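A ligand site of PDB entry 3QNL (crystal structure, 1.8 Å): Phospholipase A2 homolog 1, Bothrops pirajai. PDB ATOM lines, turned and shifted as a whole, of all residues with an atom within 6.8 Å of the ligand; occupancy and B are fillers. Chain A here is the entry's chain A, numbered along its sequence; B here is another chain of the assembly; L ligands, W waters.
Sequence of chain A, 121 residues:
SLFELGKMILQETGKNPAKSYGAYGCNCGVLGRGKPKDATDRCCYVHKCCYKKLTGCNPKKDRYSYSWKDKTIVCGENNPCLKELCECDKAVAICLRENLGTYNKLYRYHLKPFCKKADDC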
ATOM      1  N   LEU A   2     -28.414  17.804  14.207  1.00  0.00           N
ATOM      2  CA  LEU A   2     -28.054  17.900  12.803  1.00  0.00           C
ATOM      3  C   LEU A   2     -26.579  17.685  12.541  1.00  0.00           C
ATOM      4  O   LEU A   2     -26.208  17.208  11.460  1.00  0.00           O
ATOM      5  CB  LEU A   2     -28.468  19.285  12.250  1.00  0.00           C
ATOM      6  CG  LEU A   2     -29.942  19.378  11.861  1.00  0.00           C
ATOM      7  CD1 LEU A   2     -30.405  18.349  10.860  1.00  0.00           C
ATOM      8  CD2 LEU A   2     -30.843  19.400  13.100  1.00  0.00           C
ATOM      9  N   PHE A   3     -25.725  18.059  13.498  1.00  0.00           N
ATOM     10  CA  PHE A   3     -24.274  17.789  13.350  1.00  0.00           C
ATOM     11  C   PHE A   3     -24.019  16.293  13.139  1.00  0.00           C
ATOM     12  O   PHE A   3     -23.298  15.900  12.199  1.00  0.00           O
ATOM     13  CB  PHE A   3     -23.504  18.275  14.598  1.00  0.00           C
ATOM     14  CG  PHE A   3     -23.490  19.774  14.752  1.00  0.00           C
ATOM     15  CD1 PHE A   3     -22.608  20.571  13.983  1.00  0.00           C
ATOM     16  CD2 PHE A   3     -24.348  20.437  15.683  1.00  0.00           C
ATOM     17  CE1 PHE A   3     -22.586  22.035  14.173  1.00  0.00           C
ATOM     18  CE2 PHE A   3     -24.297  21.835  15.831  1.00  0.00           C
ATOM     19  CZ  PHE A   3     -23.420  22.606  15.081  1.00  0.00           C
ATOM     20  N   GLU A   4     -24.545  15.452  14.045  1.00  0.00           N
ATOM     21  CA  GLU A   4     -24.281  14.027  13.964  1.00  0.00           C
ATOM     22  C   GLU A   4     -24.967  13.439  12.682  1.00  0.00           C
ATOM     23  O   GLU A   4     -24.349  12.632  11.936  1.00  0.00           O
ATOM     24  CB  GLU A   4     -24.857  13.290  15.179  1.00  0.00           C
ATOM     25  CG  GLU A   4     -24.068  13.513  16.517  1.00  0.00           C
ATOM     26  CD  GLU A   4     -24.435  14.838  17.189  1.00  0.00           C
ATOM     27  OE1 GLU A   4     -25.483  15.468  16.886  1.00  0.00           O
ATOM     28  OE2 GLU A   4     -23.705  15.245  18.115  1.00  0.00           O
ATOM     29  N   LEU A   5     -26.208  13.887  12.427  1.00  0.00           N
ATOM     30  CA  LEU A   5     -26.965  13.372  11.278  1.00  0.00           C
ATOM     31  C   LEU A   5     -26.223  13.685   9.965  1.00  0.00           C
ATOM     32  O   LEU A   5     -26.050  12.814   9.070  1.00  0.00           O
ATOM     33  CB  LEU A   5     -28.371  14.029  11.246  1.00  0.00           C
ATOM     34  CG  LEU A   5     -29.158  13.815   9.930  1.00  0.00           C
ATOM     35  CD1 LEU A   5     -29.449  12.280   9.718  1.00  0.00           C
ATOM     36  CD2 LEU A   5     -30.473  14.625   9.971  1.00  0.00           C
ATOM     37  N   GLY A   6     -25.737  14.915   9.848  1.00  0.00           N
ATOM     38  CA  GLY A   6     -25.040  15.262   8.641  1.00  0.00           C
ATOM     39  C   GLY A   6     -23.702  14.522   8.497  1.00  0.00           C
ATOM     40  O   GLY A   6     -23.343  14.067   7.382  1.00  0.00           O
ATOM     41  N   LYS A   7     -22.990  14.354   9.598  1.00  0.00           N
ATOM     42  CA  LYS A   7     -21.765  13.528   9.569  1.00  0.00           C
ATOM     43  C   LYS A   7     -22.046  12.086   9.108  1.00  0.00           C
ATOM     44  O   LYS A   7     -21.342  11.544   8.246  1.00  0.00           O
ATOM     45  CB  LYS A   7     -21.048  13.571  10.898  1.00  0.00           C
ATOM     46  CG  LYS A   7     -19.599  13.030  10.761  1.00  0.00           C
ATOM     47  CD  LYS A   7     -18.899  13.062  12.140  1.00  0.00           C
ATOM     48  CE  LYS A   7     -17.583  12.279  12.021  1.00  0.00           C
ATOM     49  NZ  LYS A   7     -16.578  12.540  13.081  1.00  0.00           N
ATOM     50  N   MET A   8     -23.052  11.466   9.684  1.00  0.00           N
ATOM     51  CA  MET A   8     -23.455  10.093   9.248  1.00  0.00           C
ATOM     52  C   MET A   8     -23.793   9.991   7.752  1.00  0.00           C
ATOM     53  O   MET A   8     -23.441   9.016   7.113  1.00  0.00           O
ATOM     54  CB  MET A   8     -24.680   9.635  10.019  1.00  0.00           C
ATOM     55  CG  MET A   8     -24.418   9.384  11.546  1.00  0.00           C
ATOM     56  SD  MET A   8     -25.954   8.709  12.218  1.00  0.00           S
ATOM     57  CE  MET A   8     -25.472   8.660  13.926  1.00  0.00           C
ATOM     58  N   ILE A   9     -24.506  10.967   7.193  1.00  0.00           N
ATOM     59  CA  ILE A   9     -24.900  10.897   5.823  1.00  0.00           C
ATOM     60  C   ILE A   9     -23.622  11.052   5.009  1.00  0.00           C
ATOM     61  O   ILE A   9     -23.454  10.358   4.027  1.00  0.00           O
ATOM     62  CB  ILE A   9     -25.921  12.036   5.500  1.00  0.00           C
ATOM     63  CG1 ILE A   9     -27.238  11.718   6.156  1.00  0.00           C
ATOM     64  CG2 ILE A   9     -26.107  12.211   3.899  1.00  0.00           C
ATOM     65  CD1 ILE A   9     -28.268  12.929   6.159  1.00  0.00           C
ATOM     66  N   LEU A  10     -22.709  11.923   5.423  1.00  0.00           N
ATOM     67  CA  LEU A  10     -21.436  12.032   4.713  1.00  0.00           C
ATOM     68  C   LEU A  10     -20.638  10.689   4.767  1.00  0.00           C
ATOM     69  O   LEU A  10     -20.112  10.215   3.722  1.00  0.00           O
ATOM     70  CB  LEU A  10     -20.631  13.241   5.273  1.00  0.00           C
ATOM     71  CG  LEU A  10     -19.271  13.497   4.572  1.00  0.00           C
ATOM     72  CD1 LEU A  10     -19.508  13.881   3.102  1.00  0.00           C
ATOM     73  CD2 LEU A  10     -18.497  14.604   5.374  1.00  0.00           C
ATOM     74  N   GLN A  11     -20.553  10.091   5.938  1.00  0.00           N
ATOM     75  CA  GLN A  11     -19.771   8.847   6.095  1.00  0.00           C
ATOM     76  C   GLN A  11     -20.366   7.727   5.248  1.00  0.00           C
ATOM     77  O   GLN A  11     -19.607   7.015   4.652  1.00  0.00           O
ATOM     78  CB  GLN A  11     -19.693   8.405   7.556  1.00  0.00           C
ATOM     79  CG  GLN A  11     -18.802   9.417   8.354  1.00  0.00           C
ATOM     80  CD  GLN A  11     -18.907   9.190   9.919  1.00  0.00           C
ATOM     81  OE1 GLN A  11     -17.931   9.083  10.567  1.00  0.00           O
ATOM     82  NE2 GLN A  11     -20.073   9.026  10.436  1.00  0.00           N
ATOM     83  N   GLU A  12     -21.721   7.629   5.238  1.00  0.00           N
ATOM     84  CA  GLU A  12     -22.379   6.547   4.489  1.00  0.00           C
ATOM     85  C   GLU A  12     -22.366   6.837   2.979  1.00  0.00           C
ATOM     86  O   GLU A  12     -21.965   5.953   2.172  1.00  0.00           O
ATOM     87  CB  GLU A  12     -23.831   6.327   4.958  1.00  0.00           C
ATOM     88  CG  GLU A  12     -23.961   5.588   6.331  1.00  0.00           C
ATOM     89  CD  GLU A  12     -23.654   4.134   6.172  1.00  0.00           C
ATOM     90  OE1 GLU A  12     -23.884   3.609   5.060  1.00  0.00           O
ATOM     91  OE2 GLU A  12     -23.201   3.518   7.169  1.00  0.00           O
ATOM     92  N   THR A  13     -22.822   8.022   2.576  1.00  0.00           N
ATOM     93  CA  THR A  13     -23.082   8.276   1.137  1.00  0.00           C
ATOM     94  C   THR A  13     -21.864   8.829   0.402  1.00  0.00           C
ATOM     95  O   THR A  13     -21.760   8.769  -0.837  1.00  0.00           O
ATOM     96  CB  THR A  13     -24.231   9.295   0.922  1.00  0.00           C
ATOM     97  OG1 THR A  13     -23.850  10.584   1.409  1.00  0.00           O
ATOM     98  CG2 THR A  13     -25.512   8.800   1.559  1.00  0.00           C
ATOM     99  N   GLY A  14     -20.884   9.508   1.117  1.00  0.00           N
ATOM    100  CA  GLY A  14     -19.774  10.243   0.455  1.00  0.00           C
ATOM    101  C   GLY A  14     -20.259  11.585  -0.135  1.00  0.00           C
ATOM    102  O   GLY A  14     -19.490  12.257  -0.805  1.00  0.00           O
ATOM    103  N   LYS A  15     -21.518  11.943   0.108  1.00  0.00           N
ATOM    104  CA  LYS A  15     -22.104  13.170  -0.450  1.00  0.00           C
ATOM    105  C   LYS A  15     -22.221  14.283   0.560  1.00  0.00           C
ATOM    106  O   LYS A  15     -22.525  13.997   1.694  1.00  0.00           O
ATOM    107  CB  LYS A  15     -23.533  12.890  -0.924  1.00  0.00           C
ATOM    108  CG  LYS A  15     -23.684  11.863  -2.065  1.00  0.00           C
ATOM    109  CD  LYS A  15     -22.969  12.309  -3.328  1.00  0.00           C
ATOM    110  CE  LYS A  15     -23.091  11.215  -4.401  1.00  0.00           C
ATOM    111  NZ  LYS A  15     -22.779  11.728  -5.787  1.00  0.00           N
ATOM    112  N   PRO A  17     -24.126  16.530   2.708  1.00  0.00           N
ATOM    113  CA  PRO A  17     -25.541  16.300   3.053  1.00  0.00           C
ATOM    114  C   PRO A  17     -26.456  17.482   2.790  1.00  0.00           C
ATOM    115  O   PRO A  17     -27.600  17.293   2.292  1.00  0.00           O
ATOM    116  CB  PRO A  17     -25.502  15.942   4.564  1.00  0.00           C
ATOM    117  CG  PRO A  17     -24.166  16.321   5.019  1.00  0.00           C
ATOM    118  CD  PRO A  17     -23.236  16.261   3.842  1.00  0.00           C
ATOM    119  N   ARG A  63     -27.041  16.868  21.185  1.00  0.00           N
ATOM    120  CA  ARG A  63     -25.897  16.129  20.629  1.00  0.00           C
ATOM    121  C   ARG A  63     -25.879  14.729  21.258  1.00  0.00           C
ATOM    122  O   ARG A  63     -26.455  14.500  22.322  1.00  0.00           O
ATOM    123  CB  ARG A  63     -24.603  16.803  21.032  1.00  0.00           C
ATOM    124  CG  ARG A  63     -24.566  18.304  20.823  1.00  0.00           C
ATOM    125  CD  ARG A  63     -24.577  18.686  19.335  1.00  0.00           C
ATOM    126  NE  ARG A  63     -23.525  17.988  18.594  1.00  0.00           N
ATOM    127  CZ  ARG A  63     -22.403  18.577  18.228  1.00  0.00           C
ATOM    128  NH1 ARG A  63     -22.164  19.868  18.565  1.00  0.00           N
ATOM    129  NH2 ARG A  63     -21.504  17.888  17.545  1.00  0.00           N
ATOM    130  N   TRP A  68     -17.500   5.398  14.455  1.00  0.00           N
ATOM    131  CA  TRP A  68     -17.424   4.752  13.152  1.00  0.00           C
ATOM    132  C   TRP A  68     -16.449   3.613  13.431  1.00  0.00           C
ATOM    133  O   TRP A  68     -15.257   3.846  13.669  1.00  0.00           O
ATOM    134  CB  TRP A  68     -16.838   5.769  12.188  1.00  0.00           C
ATOM    135  CG  TRP A  68     -16.614   5.407  10.769  1.00  0.00           C
ATOM    136  CD1 TRP A  68     -15.409   5.351  10.117  1.00  0.00           C
ATOM    137  CD2 TRP A  68     -17.625   5.192   9.765  1.00  0.00           C
ATOM    138  NE1 TRP A  68     -15.622   5.042   8.752  1.00  0.00           N
ATOM    139  CE2 TRP A  68     -16.966   4.968   8.526  1.00  0.00           C
ATOM    140  CE3 TRP A  68     -19.038   5.124   9.793  1.00  0.00           C
ATOM    141  CZ2 TRP A  68     -17.662   4.727   7.336  1.00  0.00           C
ATOM    142  CZ3 TRP A  68     -19.700   4.857   8.592  1.00  0.00           C
ATOM    143  CH2 TRP A  68     -19.011   4.695   7.391  1.00  0.00           C
ATOM    144  N   LEU B 111     -19.274  24.392   5.537  1.00  0.00           N
ATOM    145  CA  LEU B 111     -18.915  23.616   6.761  1.00  0.00           C
ATOM    146  C   LEU B 111     -19.184  24.306   8.080  1.00  0.00           C
ATOM    147  O   LEU B 111     -18.238  24.833   8.746  1.00  0.00           O
ATOM    148  CB  LEU B 111     -17.449  23.173   6.751  1.00  0.00           C
ATOM    149  CG  LEU B 111     -17.153  21.700   6.401  1.00  0.00           C
ATOM    150  CD1 LEU B 111     -17.520  20.775   7.566  1.00  0.00           C
ATOM    151  CD2 LEU B 111     -17.773  21.239   5.046  1.00  0.00           C
ATOM    152  N   PRO B 113     -19.961  23.300  11.145  1.00  0.00           N
ATOM    153  CA  PRO B 113     -19.255  22.847  12.331  1.00  0.00           C
ATOM    154  C   PRO B 113     -17.989  23.615  12.697  1.00  0.00           C
ATOM    155  O   PRO B 113     -17.679  23.602  13.852  1.00  0.00           O
ATOM    156  CB  PRO B 113     -18.940  21.401  12.000  1.00  0.00           C
ATOM    157  CG  PRO B 113     -19.482  21.151  10.681  1.00  0.00           C
ATOM    158  CD  PRO B 113     -20.429  22.177  10.340  1.00  0.00           C
ATOM    159  N   PHE B 114     -17.285  24.238  11.766  1.00  0.00           N
ATOM    160  CA  PHE B 114     -16.072  24.979  12.091  1.00  0.00           C
ATOM    161  C   PHE B 114     -16.236  26.462  12.227  1.00  0.00           C
ATOM    162  O   PHE B 114     -15.287  27.129  12.518  1.00  0.00           O
ATOM    163  CB  PHE B 114     -14.998  24.788  11.043  1.00  0.00           C
ATOM    164  CG  PHE B 114     -14.590  23.400  10.873  1.00  0.00           C
ATOM    165  CD1 PHE B 114     -13.974  22.730  11.884  1.00  0.00           C
ATOM    166  CD2 PHE B 114     -14.842  22.755   9.703  1.00  0.00           C
ATOM    167  CE1 PHE B 114     -13.613  21.469  11.733  1.00  0.00           C
ATOM    168  CE2 PHE B 114     -14.462  21.494   9.536  1.00  0.00           C
ATOM    169  CZ  PHE B 114     -13.856  20.843  10.553  1.00  0.00           C
HETATM  170  C1  LIG L   1     -18.620  17.022  11.374  1.00  0.00           C
HETATM  171  C2  LIG L   1     -19.989  17.232  11.352  1.00  0.00           C
HETATM  172  O1  LIG L   1     -20.680  17.434  12.511  1.00  0.00           O
HETATM  173  C3  LIG L   1     -20.740  17.334  10.162  1.00  0.00           C
HETATM  174  O2  LIG L   1     -22.074  17.543  10.346  1.00  0.00           O
HETATM  175  C4  LIG L   1     -20.129  17.173   8.910  1.00  0.00           C
HETATM  176  C5  LIG L   1     -18.787  17.005   8.958  1.00  0.00           C
HETATM  177  C6  LIG L   1     -17.999  16.906  10.147  1.00  0.00           C
HETATM  178  C7  LIG L   1     -16.477  16.686  10.152  1.00  0.00           C
HETATM  179  C8  LIG L   1     -15.974  15.252   9.956  1.00  0.00           C
HETATM  180  C9  LIG L   1     -14.564  15.014  10.337  1.00  0.00           C
HETATM  181  O3  LIG L   1     -13.618  15.805   9.985  1.00  0.00           O
HETATM  182  O4  LIG L   1     -14.301  13.944  10.975  1.00  0.00           O
HETATM  183  O5  LIG L   1     -15.994  15.001   8.552  1.00  0.00           O
HETATM  184  C10 LIG L   1     -15.796  13.608   8.322  1.00  0.00           C
HETATM  185  O6  LIG L   1     -15.333  12.879   9.200  1.00  0.00           O
HETATM  186  C11 LIG L   1     -16.065  13.140   6.972  1.00  0.00           C
HETATM  187  C12 LIG L   1     -15.524  11.989   6.627  1.00  0.00           C
HETATM  188  C13 LIG L   1     -15.861  11.781   5.238  1.00  0.00           C
HETATM  189  C14 LIG L   1     -16.413  10.615   4.922  1.00  0.00           C
HETATM  190  C15 LIG L   1     -16.708  10.476   3.597  1.00  0.00           C
HETATM  191  O7  LIG L   1     -17.344   9.320   3.273  1.00  0.00           O
HETATM  192  C16 LIG L   1     -16.425  11.545   2.622  1.00  0.00           C
HETATM  193  O8  LIG L   1     -16.748  11.347   1.347  1.00  0.00           O
HETATM  194  C17 LIG L   1     -15.819  12.758   2.966  1.00  0.00           C
HETATM  195  C18 LIG L   1     -15.532  12.807   4.333  1.00  0.00           C
HETATM  196  O   HOH W   1     -11.301  14.854  10.683  1.00  0.00           O
HETATM  197  O   HOH W   2     -24.351  19.076   9.155  1.00  0.00           O
HETATM  198  O   HOH W   3     -16.829   7.471   5.414  1.00  0.00           O
HETATM  199  O   HOH W   4     -20.673  15.595  14.894  1.00  0.00           O
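Gly 6 touches the ligand. Gln 11 touches the ligand (O to O7, 3.5 Å). Gly 14 touches the ligand.
The backbone carbonyl oxygen (O) of Phe 3 is in hydrogen-bond range of an oxygen (O2) of the ligand. An oxygen (O7) of the ligand lies within hydrogen-bond range of the backbone carbonyl oxygen (O) of Leu 10 (2.9 Å). The backbone NH of Lys 7 sits at hydrogen-bond distance from an oxygen (O2) of the ligand, at 3.4 Å. An oxygen (O4) of the ligand is in salt-bridge range of the side-chain amino group of Lys 7, 3.4 Å away.
Water W3 lies within hydrogen-bond range of an oxygen (O7) of the ligand (2.9 Å) and the backbone carbonyl oxygen (O) of Gln 11 (2.9 Å).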
